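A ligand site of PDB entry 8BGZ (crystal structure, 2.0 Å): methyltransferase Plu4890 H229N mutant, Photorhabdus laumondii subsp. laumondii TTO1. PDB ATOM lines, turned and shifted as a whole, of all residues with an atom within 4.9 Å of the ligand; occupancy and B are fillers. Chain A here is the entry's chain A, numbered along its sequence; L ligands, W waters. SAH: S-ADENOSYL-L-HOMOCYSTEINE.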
ATOM      1  N   PHE A 127      -6.657 -31.786 -13.270  1.00  0.00           N
ATOM      2  CA  PHE A 127      -6.140 -30.881 -12.207  1.00  0.00           C
ATOM      3  C   PHE A 127      -6.160 -31.601 -10.847  1.00  0.00           C
ATOM      4  O   PHE A 127      -5.216 -31.387 -10.068  1.00  0.00           O
ATOM      5  CB  PHE A 127      -6.902 -29.554 -12.197  1.00  0.00           C
ATOM      6  CG  PHE A 127      -6.590 -28.693 -13.398  1.00  0.00           C
ATOM      7  CD1 PHE A 127      -5.294 -28.258 -13.618  1.00  0.00           C
ATOM      8  CD2 PHE A 127      -7.572 -28.345 -14.297  1.00  0.00           C
ATOM      9  CE1 PHE A 127      -4.996 -27.478 -14.730  1.00  0.00           C
ATOM     10  CE2 PHE A 127      -7.274 -27.564 -15.409  1.00  0.00           C
ATOM     11  CZ  PHE A 127      -5.984 -27.128 -15.617  1.00  0.00           C
ATOM     12  N   PHE A 140       3.678 -28.639 -15.867  1.00  0.00           N
ATOM     13  CA  PHE A 140       2.483 -27.915 -16.375  1.00  0.00           C
ATOM     14  C   PHE A 140       2.488 -26.471 -15.836  1.00  0.00           C
ATOM     15  O   PHE A 140       2.309 -25.541 -16.636  1.00  0.00           O
ATOM     16  CB  PHE A 140       1.186 -28.636 -15.988  1.00  0.00           C
ATOM     17  CG  PHE A 140      -0.052 -27.961 -16.511  1.00  0.00           C
ATOM     18  CD1 PHE A 140      -0.538 -28.271 -17.776  1.00  0.00           C
ATOM     19  CD2 PHE A 140      -0.711 -26.987 -15.779  1.00  0.00           C
ATOM     20  CE1 PHE A 140      -1.669 -27.641 -18.281  1.00  0.00           C
ATOM     21  CE2 PHE A 140      -1.833 -26.352 -16.280  1.00  0.00           C
ATOM     22  CZ  PHE A 140      -2.317 -26.687 -17.525  1.00  0.00           C
ATOM     23  N   ASP A 141       2.669 -26.318 -14.522  1.00  0.00           N
ATOM     24  CA  ASP A 141       2.711 -24.997 -13.832  1.00  0.00           C
ATOM     25  C   ASP A 141       3.878 -24.172 -14.381  1.00  0.00           C
ATOM     26  O   ASP A 141       3.711 -22.942 -14.496  1.00  0.00           O
ATOM     27  CB  ASP A 141       2.783 -25.165 -12.315  1.00  0.00           C
ATOM     28  CG  ASP A 141       1.489 -25.639 -11.678  1.00  0.00           C
ATOM     29  OD1 ASP A 141       0.467 -25.704 -12.409  1.00  0.00           O
ATOM     30  OD2 ASP A 141       1.496 -25.936 -10.470  1.00  0.00           O
ATOM     31  N   MET A 144       2.874 -22.873 -18.048  1.00  0.00           N
ATOM     32  CA  MET A 144       1.892 -21.755 -17.916  1.00  0.00           C
ATOM     33  C   MET A 144       2.631 -20.477 -17.475  1.00  0.00           C
ATOM     34  O   MET A 144       2.274 -19.393 -17.975  1.00  0.00           O
ATOM     35  CB  MET A 144       0.801 -22.086 -16.895  1.00  0.00           C
ATOM     36  CG  MET A 144      -0.125 -23.218 -17.303  1.00  0.00           C
ATOM     37  SD  MET A 144      -0.856 -23.025 -18.964  1.00  0.00           S
ATOM     38  CE  MET A 144       0.215 -24.116 -19.893  1.00  0.00           C
ATOM     39  N   THR A 145       3.609 -20.605 -16.578  1.00  0.00           N
ATOM     40  CA  THR A 145       4.464 -19.492 -16.069  1.00  0.00           C
ATOM     41  C   THR A 145       5.225 -18.860 -17.246  1.00  0.00           C
ATOM     42  O   THR A 145       5.244 -17.621 -17.334  1.00  0.00           O
ATOM     43  CB  THR A 145       5.383 -19.976 -14.939  1.00  0.00           C
ATOM     44  OG1 THR A 145       4.592 -20.191 -13.776  1.00  0.00           O
ATOM     45  CG2 THR A 145       6.496 -18.990 -14.615  1.00  0.00           C
ATOM     46  N   VAL A 147       4.656 -18.953 -20.648  1.00  0.00           N
ATOM     47  CA  VAL A 147       3.753 -18.314 -21.652  1.00  0.00           C
ATOM     48  C   VAL A 147       3.126 -17.055 -21.046  1.00  0.00           C
ATOM     49  O   VAL A 147       2.866 -16.105 -21.817  1.00  0.00           O
ATOM     50  CB  VAL A 147       2.682 -19.284 -22.195  1.00  0.00           C
ATOM     51  CG1 VAL A 147       3.315 -20.454 -22.934  1.00  0.00           C
ATOM     52  CG2 VAL A 147       1.727 -19.762 -21.115  1.00  0.00           C
ATOM     53  N   SER A 148       2.904 -17.036 -19.725  1.00  0.00           N
ATOM     54  CA  SER A 148       2.443 -15.848 -18.966  1.00  0.00           C
ATOM     55  C   SER A 148       3.529 -14.764 -19.006  1.00  0.00           C
ATOM     56  O   SER A 148       3.173 -13.576 -19.185  1.00  0.00           O
ATOM     57  CB  SER A 148       2.085 -16.207 -17.535  1.00  0.00           C
ATOM     58  OG  SER A 148       0.921 -17.011 -17.502  1.00  0.00           O
ATOM     59  N   VAL A 170      -7.878 -14.836 -11.878  1.00  0.00           N
ATOM     60  CA  VAL A 170      -8.653 -16.064 -11.535  1.00  0.00           C
ATOM     61  C   VAL A 170      -8.052 -17.244 -12.298  1.00  0.00           C
ATOM     62  O   VAL A 170      -7.972 -17.176 -13.548  1.00  0.00           O
ATOM     63  CB  VAL A 170     -10.156 -15.879 -11.834  1.00  0.00           C
ATOM     64  CG1 VAL A 170     -10.949 -17.156 -11.614  1.00  0.00           C
ATOM     65  CG2 VAL A 170     -10.741 -14.739 -11.012  1.00  0.00           C
ATOM     66  N   GLY A 171      -7.653 -18.299 -11.574  1.00  0.00           N
ATOM     67  CA  GLY A 171      -6.859 -19.427 -12.104  1.00  0.00           C
ATOM     68  C   GLY A 171      -5.491 -18.960 -12.577  1.00  0.00           C
ATOM     69  O   GLY A 171      -5.040 -19.424 -13.634  1.00  0.00           O
ATOM     70  N   GLY A 172      -4.837 -18.086 -11.792  1.00  0.00           N
ATOM     71  CA  GLY A 172      -3.573 -17.411 -12.165  1.00  0.00           C
ATOM     72  C   GLY A 172      -2.341 -18.278 -11.941  1.00  0.00           C
ATOM     73  O   GLY A 172      -1.226 -17.787 -12.240  1.00  0.00           O
ATOM     74  N   GLY A 173      -2.523 -19.510 -11.435  1.00  0.00           N
ATOM     75  CA  GLY A 173      -1.449 -20.498 -11.265  1.00  0.00           C
ATOM     76  C   GLY A 173      -0.411 -20.053 -10.237  1.00  0.00           C
ATOM     77  O   GLY A 173      -0.806 -19.741  -9.096  1.00  0.00           O
ATOM     78  N   LEU A 193      -6.108 -16.043  -7.490  1.00  0.00           N
ATOM     79  CA  LEU A 193      -6.962 -17.175  -7.039  1.00  0.00           C
ATOM     80  C   LEU A 193      -6.635 -18.413  -7.873  1.00  0.00           C
ATOM     81  O   LEU A 193      -6.633 -18.307  -9.119  1.00  0.00           O
ATOM     82  CB  LEU A 193      -8.442 -16.783  -7.175  1.00  0.00           C
ATOM     83  CG  LEU A 193      -9.444 -17.757  -6.552  1.00  0.00           C
ATOM     84  CD1 LEU A 193     -10.690 -17.029  -6.088  1.00  0.00           C
ATOM     85  CD2 LEU A 193      -9.810 -18.871  -7.526  1.00  0.00           C
ATOM     86  N   ASP A 194      -6.376 -19.546  -7.209  1.00  0.00           N
ATOM     87  CA  ASP A 194      -6.167 -20.869  -7.847  1.00  0.00           C
ATOM     88  C   ASP A 194      -6.447 -21.951  -6.788  1.00  0.00           C
ATOM     89  O   ASP A 194      -6.936 -21.591  -5.698  1.00  0.00           O
ATOM     90  CB  ASP A 194      -4.765 -20.980  -8.445  1.00  0.00           C
ATOM     91  CG  ASP A 194      -4.675 -21.865  -9.672  1.00  0.00           C
ATOM     92  OD1 ASP A 194      -4.804 -23.095  -9.503  1.00  0.00           O
ATOM     93  OD2 ASP A 194      -4.479 -21.326 -10.783  1.00  0.00           O
ATOM     94  N   ARG A 195      -6.177 -23.214  -7.116  1.00  0.00           N
ATOM     95  CA  ARG A 195      -6.268 -24.359  -6.180  1.00  0.00           C
ATOM     96  C   ARG A 195      -4.894 -24.563  -5.539  1.00  0.00           C
ATOM     97  O   ARG A 195      -3.978 -25.030  -6.225  1.00  0.00           O
ATOM     98  CB  ARG A 195      -6.764 -25.610  -6.933  1.00  0.00           C
ATOM     99  CG  ARG A 195      -8.156 -25.462  -7.528  1.00  0.00           C
ATOM    100  CD  ARG A 195      -8.608 -26.676  -8.311  1.00  0.00           C
ATOM    101  NE  ARG A 195      -8.779 -27.854  -7.481  1.00  0.00           N
ATOM    102  CZ  ARG A 195      -7.884 -28.828  -7.322  1.00  0.00           C
ATOM    103  NH1 ARG A 195      -6.716 -28.787  -7.950  1.00  0.00           N
ATOM    104  NH2 ARG A 195      -8.152 -29.851  -6.541  1.00  0.00           N
ATOM    105  N   GLY A 210      -9.143 -20.980  -3.761  1.00  0.00           N
ATOM    106  CA  GLY A 210     -10.563 -20.851  -4.138  1.00  0.00           C
ATOM    107  C   GLY A 210     -10.989 -21.903  -5.148  1.00  0.00           C
ATOM    108  O   GLY A 210     -10.182 -22.792  -5.470  1.00  0.00           O
ATOM    109  N   ASN A 211     -12.234 -21.785  -5.613  1.00  0.00           N
ATOM    110  CA  ASN A 211     -12.866 -22.662  -6.633  1.00  0.00           C
ATOM    111  C   ASN A 211     -13.808 -21.801  -7.483  1.00  0.00           C
ATOM    112  O   ASN A 211     -14.879 -21.443  -6.979  1.00  0.00           O
ATOM    113  CB  ASN A 211     -13.594 -23.840  -5.965  1.00  0.00           C
ATOM    114  CG  ASN A 211     -14.173 -24.837  -6.953  1.00  0.00           C
ATOM    115  OD1 ASN A 211     -14.032 -24.677  -8.167  1.00  0.00           O
ATOM    116  ND2 ASN A 211     -14.829 -25.864  -6.441  1.00  0.00           N
ATOM    117  N   PHE A 212     -13.410 -21.477  -8.724  1.00  0.00           N
ATOM    118  CA  PHE A 212     -14.173 -20.559  -9.611  1.00  0.00           C
ATOM    119  C   PHE A 212     -15.448 -21.242 -10.121  1.00  0.00           C
ATOM    120  O   PHE A 212     -16.307 -20.528 -10.684  1.00  0.00           O
ATOM    121  CB  PHE A 212     -13.302 -19.995 -10.750  1.00  0.00           C
ATOM    122  CG  PHE A 212     -12.519 -20.975 -11.596  1.00  0.00           C
ATOM    123  CD1 PHE A 212     -11.172 -20.772 -11.828  1.00  0.00           C
ATOM    124  CD2 PHE A 212     -13.134 -22.067 -12.187  1.00  0.00           C
ATOM    125  CE1 PHE A 212     -10.439 -21.639 -12.624  1.00  0.00           C
ATOM    126  CE2 PHE A 212     -12.404 -22.946 -12.966  1.00  0.00           C
ATOM    127  CZ  PHE A 212     -11.053 -22.733 -13.191  1.00  0.00           C
ATOM    128  N   LEU A 213     -15.597 -22.556  -9.929  1.00  0.00           N
ATOM    129  CA  LEU A 213     -16.852 -23.305 -10.200  1.00  0.00           C
ATOM    130  C   LEU A 213     -17.897 -22.947  -9.137  1.00  0.00           C
ATOM    131  O   LEU A 213     -19.101 -22.995  -9.445  1.00  0.00           O
ATOM    132  CB  LEU A 213     -16.584 -24.809 -10.194  1.00  0.00           C
ATOM    133  CG  LEU A 213     -15.624 -25.331 -11.273  1.00  0.00           C
ATOM    134  CD1 LEU A 213     -15.296 -26.798 -11.036  1.00  0.00           C
ATOM    135  CD2 LEU A 213     -16.199 -25.137 -12.668  1.00  0.00           C
ATOM    136  N   LYS A 226      -7.247 -15.948 -17.871  1.00  0.00           N
ATOM    137  CA  LYS A 226      -6.302 -16.253 -18.980  1.00  0.00           C
ATOM    138  C   LYS A 226      -6.061 -17.761 -19.067  1.00  0.00           C
ATOM    139  O   LYS A 226      -5.620 -18.352 -18.057  1.00  0.00           O
ATOM    140  CB  LYS A 226      -4.989 -15.493 -18.769  1.00  0.00           C
ATOM    141  CG  LYS A 226      -3.989 -15.596 -19.914  1.00  0.00           C
ATOM    142  CD  LYS A 226      -2.802 -14.687 -19.734  1.00  0.00           C
ATOM    143  CE  LYS A 226      -1.478 -15.322 -20.123  1.00  0.00           C
ATOM    144  NZ  LYS A 226      -1.133 -16.459 -19.242  1.00  0.00           N
ATOM    145  N   ASN A 227      -6.332 -18.344 -20.243  1.00  0.00           N
ATOM    146  CA  ASN A 227      -6.081 -19.775 -20.570  1.00  0.00           C
ATOM    147  C   ASN A 227      -6.731 -20.672 -19.508  1.00  0.00           C
ATOM    148  O   ASN A 227      -6.047 -21.604 -19.022  1.00  0.00           O
ATOM    149  CB  ASN A 227      -4.578 -20.063 -20.728  1.00  0.00           C
ATOM    150  CG  ASN A 227      -3.938 -19.330 -21.896  1.00  0.00           C
ATOM    151  OD1 ASN A 227      -4.582 -19.093 -22.911  1.00  0.00           O
ATOM    152  ND2 ASN A 227      -2.665 -18.988 -21.754  1.00  0.00           N
ATOM    153  N   VAL A 228      -7.997 -20.413 -19.183  1.00  0.00           N
ATOM    154  CA  VAL A 228      -8.823 -21.224 -18.240  1.00  0.00           C
ATOM    155  C   VAL A 228      -9.936 -21.921 -19.025  1.00  0.00           C
ATOM    156  O   VAL A 228     -10.007 -23.158 -18.954  1.00  0.00           O
ATOM    157  CB  VAL A 228      -9.391 -20.365 -17.086  1.00  0.00           C
ATOM    158  CG1 VAL A 228     -10.444 -21.119 -16.276  1.00  0.00           C
ATOM    159  CG2 VAL A 228      -8.291 -19.845 -16.169  1.00  0.00           C
ATOM    160  N   ASN A 231     -10.013 -25.245 -20.791  1.00  0.00           N
ATOM    161  CA  ASN A 231      -9.974 -26.462 -19.940  1.00  0.00           C
ATOM    162  C   ASN A 231     -11.395 -26.915 -19.550  1.00  0.00           C
ATOM    163  O   ASN A 231     -11.483 -27.840 -18.714  1.00  0.00           O
ATOM    164  CB  ASN A 231      -9.158 -26.238 -18.663  1.00  0.00           C
ATOM    165  CG  ASN A 231      -7.785 -25.656 -18.917  1.00  0.00           C
ATOM    166  OD1 ASN A 231      -7.207 -25.835 -19.992  1.00  0.00           O
ATOM    167  ND2 ASN A 231      -7.248 -24.951 -17.933  1.00  0.00           N
ATOM    168  N   TRP A 232     -12.453 -26.308 -20.088  1.00  0.00           N
ATOM    169  CA  TRP A 232     -13.845 -26.513 -19.616  1.00  0.00           C
ATOM    170  C   TRP A 232     -14.832 -26.625 -20.783  1.00  0.00           C
ATOM    171  O   TRP A 232     -14.586 -26.016 -21.838  1.00  0.00           O
ATOM    172  CB  TRP A 232     -14.258 -25.392 -18.652  1.00  0.00           C
ATOM    173  CG  TRP A 232     -13.357 -25.308 -17.452  1.00  0.00           C
ATOM    174  CD1 TRP A 232     -12.331 -24.430 -17.276  1.00  0.00           C
ATOM    175  CD2 TRP A 232     -13.365 -26.165 -16.301  1.00  0.00           C
ATOM    176  NE1 TRP A 232     -11.705 -24.671 -16.081  1.00  0.00           N
ATOM    177  CE2 TRP A 232     -12.320 -25.732 -15.465  1.00  0.00           C
ATOM    178  CE3 TRP A 232     -14.160 -27.253 -15.897  1.00  0.00           C
ATOM    179  CZ2 TRP A 232     -12.046 -26.345 -14.242  1.00  0.00           C
ATOM    180  CZ3 TRP A 232     -13.884 -27.854 -14.690  1.00  0.00           C
ATOM    181  CH2 TRP A 232     -12.851 -27.405 -13.870  1.00  0.00           C
HETATM  182  N   SAH L   1      -3.940 -18.442 -15.943  1.00  0.00           N
HETATM  183  CA  SAH L   1      -2.629 -19.166 -15.940  1.00  0.00           C
HETATM  184  CB  SAH L   1      -2.807 -20.681 -15.796  1.00  0.00           C
HETATM  185  CG  SAH L   1      -3.920 -21.270 -16.640  1.00  0.00           C
HETATM  186  SD  SAH L   1      -3.950 -23.081 -16.604  1.00  0.00           S
HETATM  187  C   SAH L   1      -1.884 -18.867 -17.246  1.00  0.00           C
HETATM  188  O   SAH L   1      -0.674 -19.024 -17.332  1.00  0.00           O
HETATM  189  OXT SAH L   1      -2.489 -18.467 -18.251  1.00  0.00           O
HETATM  190  C5' SAH L   1      -5.476 -23.376 -15.681  1.00  0.00           C
HETATM  191  C4' SAH L   1      -5.363 -22.971 -14.230  1.00  0.00           C
HETATM  192  O4' SAH L   1      -6.660 -23.094 -13.602  1.00  0.00           O
HETATM  193  C3' SAH L   1      -4.400 -23.831 -13.402  1.00  0.00           C
HETATM  194  O3' SAH L   1      -3.521 -23.012 -12.643  1.00  0.00           O
HETATM  195  C2' SAH L   1      -5.336 -24.656 -12.519  1.00  0.00           C
HETATM  196  O2' SAH L   1      -4.733 -25.028 -11.296  1.00  0.00           O
HETATM  197  C1' SAH L   1      -6.479 -23.678 -12.333  1.00  0.00           C
HETATM  198  N9  SAH L   1      -7.735 -24.273 -11.901  1.00  0.00           N
HETATM  199  C8  SAH L   1      -8.307 -25.436 -12.353  1.00  0.00           C
HETATM  200  N7  SAH L   1      -9.456 -25.708 -11.802  1.00  0.00           N
HETATM  201  C5  SAH L   1      -9.670 -24.647 -10.932  1.00  0.00           C
HETATM  202  C6  SAH L   1     -10.731 -24.342 -10.046  1.00  0.00           C
HETATM  203  N6  SAH L   1     -11.806 -25.109  -9.902  1.00  0.00           N
HETATM  204  N1  SAH L   1     -10.636 -23.201  -9.318  1.00  0.00           N
HETATM  205  C2  SAH L   1      -9.549 -22.437  -9.488  1.00  0.00           C
HETATM  206  N3  SAH L   1      -8.495 -22.615 -10.273  1.00  0.00           N
HETATM  207  C4  SAH L   1      -8.619 -23.756 -10.991  1.00  0.00           C
HETATM  208  O   HOH W   1     -10.388 -28.316 -11.043  1.00  0.00           O
HETATM  209  O   HOH W   2      -0.719 -23.271 -13.607  1.00  0.00           O
HETATM  210  O   HOH W   3      -8.714 -24.241 -15.470  1.00  0.00           O
HETATM  211  O   HOH W   4       0.537 -19.252 -14.814  1.00  0.00           O
HETATM  212  O   HOH W   5      -6.057 -16.309 -15.277  1.00  0.00           O
HETATM  213  O   HOH W   6      -2.004 -26.735 -11.131  1.00  0.00           O
HETATM  214  O   HOH W   7      -2.599 -15.896 -15.576  1.00  0.00           O
HETATM  215  O   HOH W   8      -5.191 -27.128  -9.800  1.00  0.00           O
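The backbone carbonyl oxygen of Met 144 lies close to an oxygen (O) of the ligand (3.0 Å). The backbone carbonyl oxygen of Gly 171 is in hydrogen-bond range of a nitrogen (N) of the ligand, at 2.7 Å. A nitrogen (N6) of the ligand lies within hydrogen-bond range of the side-chain amide oxygen (OD1) of Asn 211 (2.9 Å). A nitrogen (N1) of the ligand is in hydrogen-bond range of the backbone NH of Phe 212 (3.3 Å). A nitrogen (N) of the ligand sits at hydrogen-bond distance from the backbone carbonyl oxygen (O) of Lys 226 (2.7 Å). OD1 of Asp 194 sits at hydrogen-bond distance from O2' of the ligand, at 2.6 Å. An oxygen (O) of the ligand sits at hydrogen-bond distance from the side-chain hydroxyl (OG) of Ser 148. OXT of the ligand lies within salt-bridge range of NZ of Lys 226, at 2.6 Å.
O of Leu 193 sits at hydrogen-bond distance from N of Gly 171 (2.7 Å). O of Asp 194 lies within hydrogen-bond range of N of Gly 210 (3.0 Å). OG of Ser 148 sits at hydrogen-bond distance from NZ of Lys 226 (2.7 Å). The backbone carbonyl oxygen (O) of Val 228 sits close to the side-chain amide nitrogen (ND2) of Asn 231 (3.4 Å). O of Met 144 sits at hydrogen-bond distance from OG of Ser 148, at 2.8 Å. The side-chain carboxylate (OD2) of Asp 194 lies within hydrogen-bond range of the backbone NH (N) of Gly 173, at 2.7 Å. The side-chain amide oxygen of Asn 211 lies close to the backbone NH of Leu 213 (3.2 Å). The side-chain carboxylate (OD2) of Asp 194 is in hydrogen-bond range of the backbone NH (N) of Gly 172.
SD of the ligand sits close to O of Asn 227, 3.5 Å away. Merely in contact with the ligand: Phe 127 (3.6 Å), Phe 140 (3.9 Å), Gly 172 (3.9 Å), Gly 173 (3.5 Å), Arg 195 (3.5 Å), Gly 210 (3.9 Å), Asn 231 (3.3 Å) and Trp 232 (3.6 Å). Hydrophobic or aromatic side chains within 4 Å of the ligand: Phe 127, Phe 140, Met 144, Phe 212 and Trp 232. 16 residues have an atom within 4 Å of the ligand: Phe 127, Phe 140, Met 144, Ser 148, Gly 171, Gly 172, Gly 173, Asp 194, Arg 195, Gly 210, Asn 211, Phe 212, Lys 226, Asn 227, Asn 231 and Trp 232.
Water W8 lies within hydrogen-bond range of an oxygen (O2') of the ligand and the guanidinium group of Arg 195. Water W4 bridges an oxygen (O) of the ligand (2.8 Å) and the backbone carbonyl oxygen of Gly 172 (3.4 Å). Water W2 bridges OD1 of Asp 141 and O3' of the ligand. Water W3 lies within hydrogen-bond range of ND2 of Asn 231, O4' of the ligand and NE1 of Trp 232. Water W5 lies within hydrogen-bond range of the backbone carbonyl oxygen (O) of Val 170 (2.7 Å), the backbone NH (N) of Lys 226 (2.9 Å) and a nitrogen (N) of the ligand (3.1 Å). Water W6 lies within hydrogen-bond range of the side-chain carboxylate of Asp 141 and an oxygen (O2') of the ligand.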
